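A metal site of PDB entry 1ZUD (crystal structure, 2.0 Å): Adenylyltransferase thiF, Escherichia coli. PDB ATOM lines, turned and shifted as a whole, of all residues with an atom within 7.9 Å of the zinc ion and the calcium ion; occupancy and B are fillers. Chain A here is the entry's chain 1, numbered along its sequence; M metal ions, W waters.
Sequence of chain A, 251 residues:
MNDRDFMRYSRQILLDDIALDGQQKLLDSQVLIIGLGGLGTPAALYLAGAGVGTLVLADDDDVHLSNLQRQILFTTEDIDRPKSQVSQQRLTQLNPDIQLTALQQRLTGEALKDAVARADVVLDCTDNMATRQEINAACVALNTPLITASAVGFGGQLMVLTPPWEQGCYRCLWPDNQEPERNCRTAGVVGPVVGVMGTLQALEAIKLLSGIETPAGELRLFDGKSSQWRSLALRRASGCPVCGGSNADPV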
ATOM      1  N   ASN A 136       0.534 -24.689   9.987  1.00  0.00           N
ATOM      2  CA  ASN A 136       1.441 -24.746  11.129  1.00  0.00           C
ATOM      3  C   ASN A 136       0.683 -25.282  12.375  1.00  0.00           C
ATOM      4  O   ASN A 136       1.204 -26.125  13.129  1.00  0.00           O
ATOM      5  CB  ASN A 136       1.992 -23.333  11.393  1.00  0.00           C
ATOM      6  CG  ASN A 136       2.799 -23.243  12.704  1.00  0.00           C
ATOM      7  OD1 ASN A 136       3.911 -23.745  12.807  1.00  0.00           O
ATOM      8  ND2 ASN A 136       2.232 -22.587  13.699  1.00  0.00           N
ATOM      9  N   VAL A 140       1.896 -28.853  14.406  1.00  0.00           N
ATOM     10  CA  VAL A 140       2.256 -28.922  15.818  1.00  0.00           C
ATOM     11  C   VAL A 140       1.271 -29.878  16.583  1.00  0.00           C
ATOM     12  O   VAL A 140       1.689 -30.809  17.296  1.00  0.00           O
ATOM     13  CB  VAL A 140       2.245 -27.509  16.440  1.00  0.00           C
ATOM     14  CG1 VAL A 140       2.588 -27.580  17.931  1.00  0.00           C
ATOM     15  CG2 VAL A 140       3.313 -26.613  15.672  1.00  0.00           C
ATOM     16  N   PRO A 164      10.525 -31.548  19.227  1.00  0.00           N
ATOM     17  CA  PRO A 164       9.574 -30.991  20.190  1.00  0.00           C
ATOM     18  C   PRO A 164       9.389 -29.449  20.120  1.00  0.00           C
ATOM     19  O   PRO A 164       9.100 -28.805  21.119  1.00  0.00           O
ATOM     20  CB  PRO A 164      10.159 -31.477  21.533  1.00  0.00           C
ATOM     21  CG  PRO A 164      11.689 -31.196  21.338  1.00  0.00           C
ATOM     22  CD  PRO A 164      11.905 -31.554  19.796  1.00  0.00           C
ATOM     23  N   TRP A 165       9.564 -28.865  18.931  1.00  0.00           N
ATOM     24  CA  TRP A 165       9.382 -27.414  18.714  1.00  0.00           C
ATOM     25  C   TRP A 165      10.187 -26.534  19.685  1.00  0.00           C
ATOM     26  O   TRP A 165       9.700 -25.510  20.182  1.00  0.00           O
ATOM     27  CB  TRP A 165       7.888 -27.060  18.812  1.00  0.00           C
ATOM     28  CG  TRP A 165       7.020 -28.124  18.141  1.00  0.00           C
ATOM     29  CD1 TRP A 165       6.280 -29.121  18.757  1.00  0.00           C
ATOM     30  CD2 TRP A 165       6.860 -28.316  16.733  1.00  0.00           C
ATOM     31  NE1 TRP A 165       5.664 -29.922  17.788  1.00  0.00           N
ATOM     32  CE2 TRP A 165       6.003 -29.459  16.550  1.00  0.00           C
ATOM     33  CE3 TRP A 165       7.340 -27.649  15.598  1.00  0.00           C
ATOM     34  CZ2 TRP A 165       5.622 -29.925  15.273  1.00  0.00           C
ATOM     35  CZ3 TRP A 165       6.970 -28.119  14.334  1.00  0.00           C
ATOM     36  CH2 TRP A 165       6.113 -29.253  14.182  1.00  0.00           C
ATOM     37  N   GLU A 166      11.405 -26.961  19.967  1.00  0.00           N
ATOM     38  CA  GLU A 166      12.327 -26.254  20.870  1.00  0.00           C
ATOM     39  C   GLU A 166      12.614 -24.805  20.457  1.00  0.00           C
ATOM     40  O   GLU A 166      12.890 -23.932  21.328  1.00  0.00           O
ATOM     41  CB  GLU A 166      13.650 -27.044  20.941  1.00  0.00           C
ATOM     42  CG  GLU A 166      14.681 -26.520  21.952  1.00  0.00           C
ATOM     43  CD  GLU A 166      14.271 -26.784  23.413  1.00  0.00           C
ATOM     44  OE1 GLU A 166      13.471 -27.732  23.634  1.00  0.00           O
ATOM     45  OE2 GLU A 166      14.757 -26.065  24.334  1.00  0.00           O
ATOM     46  N   GLN A 167      12.618 -24.527  19.145  1.00  0.00           N
ATOM     47  CA  GLN A 167      12.817 -23.157  18.642  1.00  0.00           C
ATOM     48  C   GLN A 167      11.460 -22.539  18.213  1.00  0.00           C
ATOM     49  O   GLN A 167      11.411 -21.624  17.424  1.00  0.00           O
ATOM     50  CB  GLN A 167      13.772 -23.153  17.444  1.00  0.00           C
ATOM     51  CG  GLN A 167      15.281 -23.073  17.832  1.00  0.00           C
ATOM     52  CD  GLN A 167      15.756 -24.284  18.554  1.00  0.00           C
ATOM     53  OE1 GLN A 167      15.723 -25.391  18.008  1.00  0.00           O
ATOM     54  NE2 GLN A 167      16.195 -24.099  19.778  1.00  0.00           N
ATOM     55  N   GLY A 168      10.359 -23.113  18.695  1.00  0.00           N
ATOM     56  CA  GLY A 168       9.067 -22.548  18.381  1.00  0.00           C
ATOM     57  C   GLY A 168       8.465 -23.004  17.064  1.00  0.00           C
ATOM     58  O   GLY A 168       8.948 -23.970  16.426  1.00  0.00           O
ATOM     59  N   CYS A 169       7.453 -22.263  16.613  1.00  0.00           N
ATOM     60  CA  CYS A 169       6.738 -22.628  15.403  1.00  0.00           C
ATOM     61  C   CYS A 169       6.578 -21.404  14.505  1.00  0.00           C
ATOM     62  O   CYS A 169       7.223 -20.348  14.710  1.00  0.00           O
ATOM     63  CB  CYS A 169       5.384 -23.242  15.799  1.00  0.00           C
ATOM     64  SG  CYS A 169       4.146 -22.064  16.403  1.00  0.00           S
ATOM     65  N   TYR A 170       5.740 -21.548  13.481  1.00  0.00           N
ATOM     66  CA  TYR A 170       5.562 -20.451  12.527  1.00  0.00           C
ATOM     67  C   TYR A 170       4.915 -19.255  13.236  1.00  0.00           C
ATOM     68  O   TYR A 170       5.274 -18.073  13.000  1.00  0.00           O
ATOM     69  CB  TYR A 170       4.692 -20.933  11.369  1.00  0.00           C
ATOM     70  CG  TYR A 170       4.557 -19.925  10.236  1.00  0.00           C
ATOM     71  CD1 TYR A 170       5.501 -19.857   9.185  1.00  0.00           C
ATOM     72  CD2 TYR A 170       3.469 -19.010  10.207  1.00  0.00           C
ATOM     73  CE1 TYR A 170       5.363 -18.913   8.130  1.00  0.00           C
ATOM     74  CE2 TYR A 170       3.336 -18.074   9.206  1.00  0.00           C
ATOM     75  CZ  TYR A 170       4.287 -18.023   8.169  1.00  0.00           C
ATOM     76  OH  TYR A 170       4.178 -17.026   7.221  1.00  0.00           O
ATOM     77  N   ARG A 171       3.980 -19.562  14.134  1.00  0.00           N
ATOM     78  CA  ARG A 171       3.275 -18.555  14.864  1.00  0.00           C
ATOM     79  C   ARG A 171       4.136 -17.851  15.897  1.00  0.00           C
ATOM     80  O   ARG A 171       3.841 -16.707  16.268  1.00  0.00           O
ATOM     81  CB  ARG A 171       2.005 -19.101  15.506  1.00  0.00           C
ATOM     82  CG  ARG A 171       1.178 -17.980  16.162  1.00  0.00           C
ATOM     83  CD  ARG A 171      -0.314 -18.215  16.114  1.00  0.00           C
ATOM     84  NE  ARG A 171      -0.905 -17.616  14.926  1.00  0.00           N
ATOM     85  CZ  ARG A 171      -2.211 -17.538  14.693  1.00  0.00           C
ATOM     86  NH1 ARG A 171      -3.064 -18.023  15.586  1.00  0.00           N
ATOM     87  NH2 ARG A 171      -2.661 -16.962  13.576  1.00  0.00           N
ATOM     88  N   CYS A 172       5.188 -18.494  16.381  1.00  0.00           N
ATOM     89  CA  CYS A 172       6.089 -17.795  17.300  1.00  0.00           C
ATOM     90  C   CYS A 172       6.847 -16.717  16.537  1.00  0.00           C
ATOM     91  O   CYS A 172       7.203 -15.665  17.102  1.00  0.00           O
ATOM     92  CB  CYS A 172       7.154 -18.727  17.855  1.00  0.00           C
ATOM     93  SG  CYS A 172       6.589 -20.009  18.989  1.00  0.00           S
ATOM     94  N   LEU A 173       7.159 -16.996  15.263  1.00  0.00           N
ATOM     95  CA  LEU A 173       7.896 -16.016  14.430  1.00  0.00           C
ATOM     96  C   LEU A 173       6.967 -14.924  13.897  1.00  0.00           C
ATOM     97  O   LEU A 173       7.296 -13.746  13.914  1.00  0.00           O
ATOM     98  CB  LEU A 173       8.588 -16.709  13.232  1.00  0.00           C
ATOM     99  CG  LEU A 173       9.269 -15.789  12.223  1.00  0.00           C
ATOM    100  CD1 LEU A 173      10.362 -14.956  12.922  1.00  0.00           C
ATOM    101  CD2 LEU A 173       9.889 -16.652  11.114  1.00  0.00           C
ATOM    102  N   TRP A 174       5.802 -15.337  13.423  1.00  0.00           N
ATOM    103  CA  TRP A 174       4.857 -14.403  12.848  1.00  0.00           C
ATOM    104  C   TRP A 174       3.566 -14.472  13.650  1.00  0.00           C
ATOM    105  O   TRP A 174       2.683 -15.306  13.403  1.00  0.00           O
ATOM    106  CB  TRP A 174       4.593 -14.758  11.384  1.00  0.00           C
ATOM    107  CG  TRP A 174       5.830 -14.755  10.522  1.00  0.00           C
ATOM    108  CD1 TRP A 174       6.332 -15.822   9.856  1.00  0.00           C
ATOM    109  CD2 TRP A 174       6.753 -13.658  10.310  1.00  0.00           C
ATOM    110  NE1 TRP A 174       7.515 -15.479   9.240  1.00  0.00           N
ATOM    111  CE2 TRP A 174       7.803 -14.161   9.504  1.00  0.00           C
ATOM    112  CE3 TRP A 174       6.807 -12.317  10.717  1.00  0.00           C
ATOM    113  CZ2 TRP A 174       8.896 -13.356   9.083  1.00  0.00           C
ATOM    114  CZ3 TRP A 174       7.907 -11.507  10.308  1.00  0.00           C
ATOM    115  CH2 TRP A 174       8.925 -12.037   9.506  1.00  0.00           C
ATOM    116  N   ARG A 235      13.323 -18.629  17.946  1.00  0.00           N
ATOM    117  CA  ARG A 235      13.187 -18.698  19.412  1.00  0.00           C
ATOM    118  C   ARG A 235      11.693 -18.906  19.735  1.00  0.00           C
ATOM    119  O   ARG A 235      10.824 -18.273  19.135  1.00  0.00           O
ATOM    120  CB  ARG A 235      13.705 -17.368  19.996  1.00  0.00           C
ATOM    121  CG  ARG A 235      13.614 -17.251  21.510  1.00  0.00           C
ATOM    122  CD  ARG A 235      14.656 -16.258  22.067  1.00  0.00           C
ATOM    123  NE  ARG A 235      14.659 -16.242  23.532  1.00  0.00           N
ATOM    124  CZ  ARG A 235      14.881 -15.149  24.275  1.00  0.00           C
ATOM    125  NH1 ARG A 235      15.133 -13.979  23.690  1.00  0.00           N
ATOM    126  NH2 ARG A 235      14.809 -15.216  25.602  1.00  0.00           N
ATOM    127  N   ARG A 236      11.373 -19.805  20.653  1.00  0.00           N
ATOM    128  CA  ARG A 236       9.928 -19.969  20.902  1.00  0.00           C
ATOM    129  C   ARG A 236       9.405 -18.769  21.737  1.00  0.00           C
ATOM    130  O   ARG A 236      10.160 -18.142  22.488  1.00  0.00           O
ATOM    131  CB  ARG A 236       9.656 -21.317  21.570  1.00  0.00           C
ATOM    132  CG  ARG A 236      10.263 -21.471  22.890  1.00  0.00           C
ATOM    133  CD  ARG A 236       9.989 -22.902  23.357  1.00  0.00           C
ATOM    134  NE  ARG A 236      10.459 -23.025  24.731  1.00  0.00           N
ATOM    135  CZ  ARG A 236      11.697 -23.369  25.073  1.00  0.00           C
ATOM    136  NH1 ARG A 236      12.586 -23.651  24.141  1.00  0.00           N
ATOM    137  NH2 ARG A 236      12.071 -23.333  26.355  1.00  0.00           N
ATOM    138  N   ALA A 237       8.154 -18.399  21.493  1.00  0.00           N
ATOM    139  CA  ALA A 237       7.479 -17.320  22.163  1.00  0.00           C
ATOM    140  C   ALA A 237       6.661 -17.958  23.308  1.00  0.00           C
ATOM    141  O   ALA A 237       5.764 -18.796  23.078  1.00  0.00           O
ATOM    142  CB  ALA A 237       6.552 -16.608  21.187  1.00  0.00           C
ATOM    143  N   SER A 238       6.923 -17.532  24.537  1.00  0.00           N
ATOM    144  CA  SER A 238       6.200 -18.131  25.683  1.00  0.00           C
ATOM    145  C   SER A 238       4.696 -18.048  25.531  1.00  0.00           C
ATOM    146  O   SER A 238       3.982 -18.997  25.848  1.00  0.00           O
ATOM    147  CB  SER A 238       6.615 -17.475  26.995  1.00  0.00           C
ATOM    148  OG  SER A 238       6.128 -16.141  27.028  1.00  0.00           O
ATOM    149  N   GLY A 239       4.195 -16.944  25.009  1.00  0.00           N
ATOM    150  CA  GLY A 239       2.742 -16.869  24.861  1.00  0.00           C
ATOM    151  C   GLY A 239       2.104 -17.527  23.656  1.00  0.00           C
ATOM    152  O   GLY A 239       0.874 -17.418  23.482  1.00  0.00           O
ATOM    153  N   CYS A 240       2.886 -18.248  22.828  1.00  0.00           N
ATOM    154  CA  CYS A 240       2.345 -18.845  21.612  1.00  0.00           C
ATOM    155  C   CYS A 240       1.123 -19.734  21.819  1.00  0.00           C
ATOM    156  O   CYS A 240       1.208 -20.756  22.513  1.00  0.00           O
ATOM    157  CB  CYS A 240       3.428 -19.636  20.840  1.00  0.00           C
ATOM    158  SG  CYS A 240       2.842 -20.173  19.233  1.00  0.00           S
ATOM    159  N   PRO A 241      -0.007 -19.380  21.172  1.00  0.00           N
ATOM    160  CA  PRO A 241      -1.263 -20.128  21.264  1.00  0.00           C
ATOM    161  C   PRO A 241      -1.182 -21.481  20.593  1.00  0.00           C
ATOM    162  O   PRO A 241      -2.089 -22.289  20.763  1.00  0.00           O
ATOM    163  CB  PRO A 241      -2.287 -19.232  20.557  1.00  0.00           C
ATOM    164  CG  PRO A 241      -1.447 -18.436  19.590  1.00  0.00           C
ATOM    165  CD  PRO A 241      -0.207 -18.121  20.416  1.00  0.00           C
ATOM    166  N   VAL A 242      -0.111 -21.732  19.822  1.00  0.00           N
ATOM    167  CA  VAL A 242       0.004 -23.021  19.145  1.00  0.00           C
ATOM    168  C   VAL A 242       0.980 -24.007  19.826  1.00  0.00           C
ATOM    169  O   VAL A 242       0.624 -25.189  20.052  1.00  0.00           O
ATOM    170  CB  VAL A 242       0.413 -22.801  17.646  1.00  0.00           C
ATOM    171  CG1 VAL A 242       0.671 -24.123  16.947  1.00  0.00           C
ATOM    172  CG2 VAL A 242      -0.652 -22.048  16.919  1.00  0.00           C
ATOM    173  N   CYS A 243       2.212 -23.556  20.107  1.00  0.00           N
ATOM    174  CA  CYS A 243       3.205 -24.459  20.703  1.00  0.00           C
ATOM    175  C   CYS A 243       3.657 -24.048  22.129  1.00  0.00           C
ATOM    176  O   CYS A 243       4.564 -24.663  22.717  1.00  0.00           O
ATOM    177  CB  CYS A 243       4.439 -24.560  19.755  1.00  0.00           C
ATOM    178  SG  CYS A 243       5.540 -23.076  19.848  1.00  0.00           S
ATOM    179  N   GLY A 244       2.997 -23.040  22.705  1.00  0.00           N
ATOM    180  CA  GLY A 244       3.390 -22.613  24.031  1.00  0.00           C
ATOM    181  C   GLY A 244       2.757 -23.443  25.170  1.00  0.00           C
ATOM    182  O   GLY A 244       3.019 -23.172  26.328  1.00  0.00           O
ATOM    183  N   GLY A 245       1.944 -24.437  24.872  1.00  0.00           N
ATOM    184  CA  GLY A 245       1.356 -25.207  25.966  1.00  0.00           C
ATOM    185  C   GLY A 245      -0.139 -25.005  26.211  1.00  0.00           C
ATOM    186  O   GLY A 245      -0.802 -25.959  26.688  1.00  0.00           O
HETATM  187 ZN    ZN M   1       4.745 -21.253  18.457  1.00  0.00          ZN
HETATM  188 CA    CA M   2       6.377 -25.675  23.584  1.00  0.00          CA
HETATM  189  O   HOH W   1       8.495 -26.067  24.573  1.00  0.00           O
HETATM  190  O   HOH W   2       6.791 -27.780  22.549  1.00  0.00           O
HETATM  191  O   HOH W   3       7.605 -24.639  21.756  1.00  0.00           O
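SG of Cys 172 sits close to N of Ala 237 (3.4 Å). SG of Cys 169 lies close to N of Arg 171, 3.4 Å away. The side-chain amide nitrogen of Asn 136 sits close to the side-chain sulfur of Cys 169, 3.4 Å away. The side-chain sulfur (SG) of Cys 240 sits close to the backbone NH (N) of Val 242, at 3.4 Å.
Of the 24 residues printed, 4 come within 4 Å of the zinc ion.
One residue has an atom within 4 Å of the calcium ion: Cys 243.
SG of Cys 172 is bound to the zinc ion, at 2.3 Å. SG of Cys 169 is bound to the zinc ion (2.3 Å). The side-chain sulfur (SG) of Cys 240 is bound to the zinc ion, 2.3 Å away. The side-chain sulfur (SG) of Cys 243 binds the zinc ion (2.4 Å).
The calcium ion is bound by O of Cys 243 (2.3 Å), water W1 (2.4 Å), water W2 (2.4 Å) and water W3 (2.4 Å). The calcium ion has four donor atoms within binding distance.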
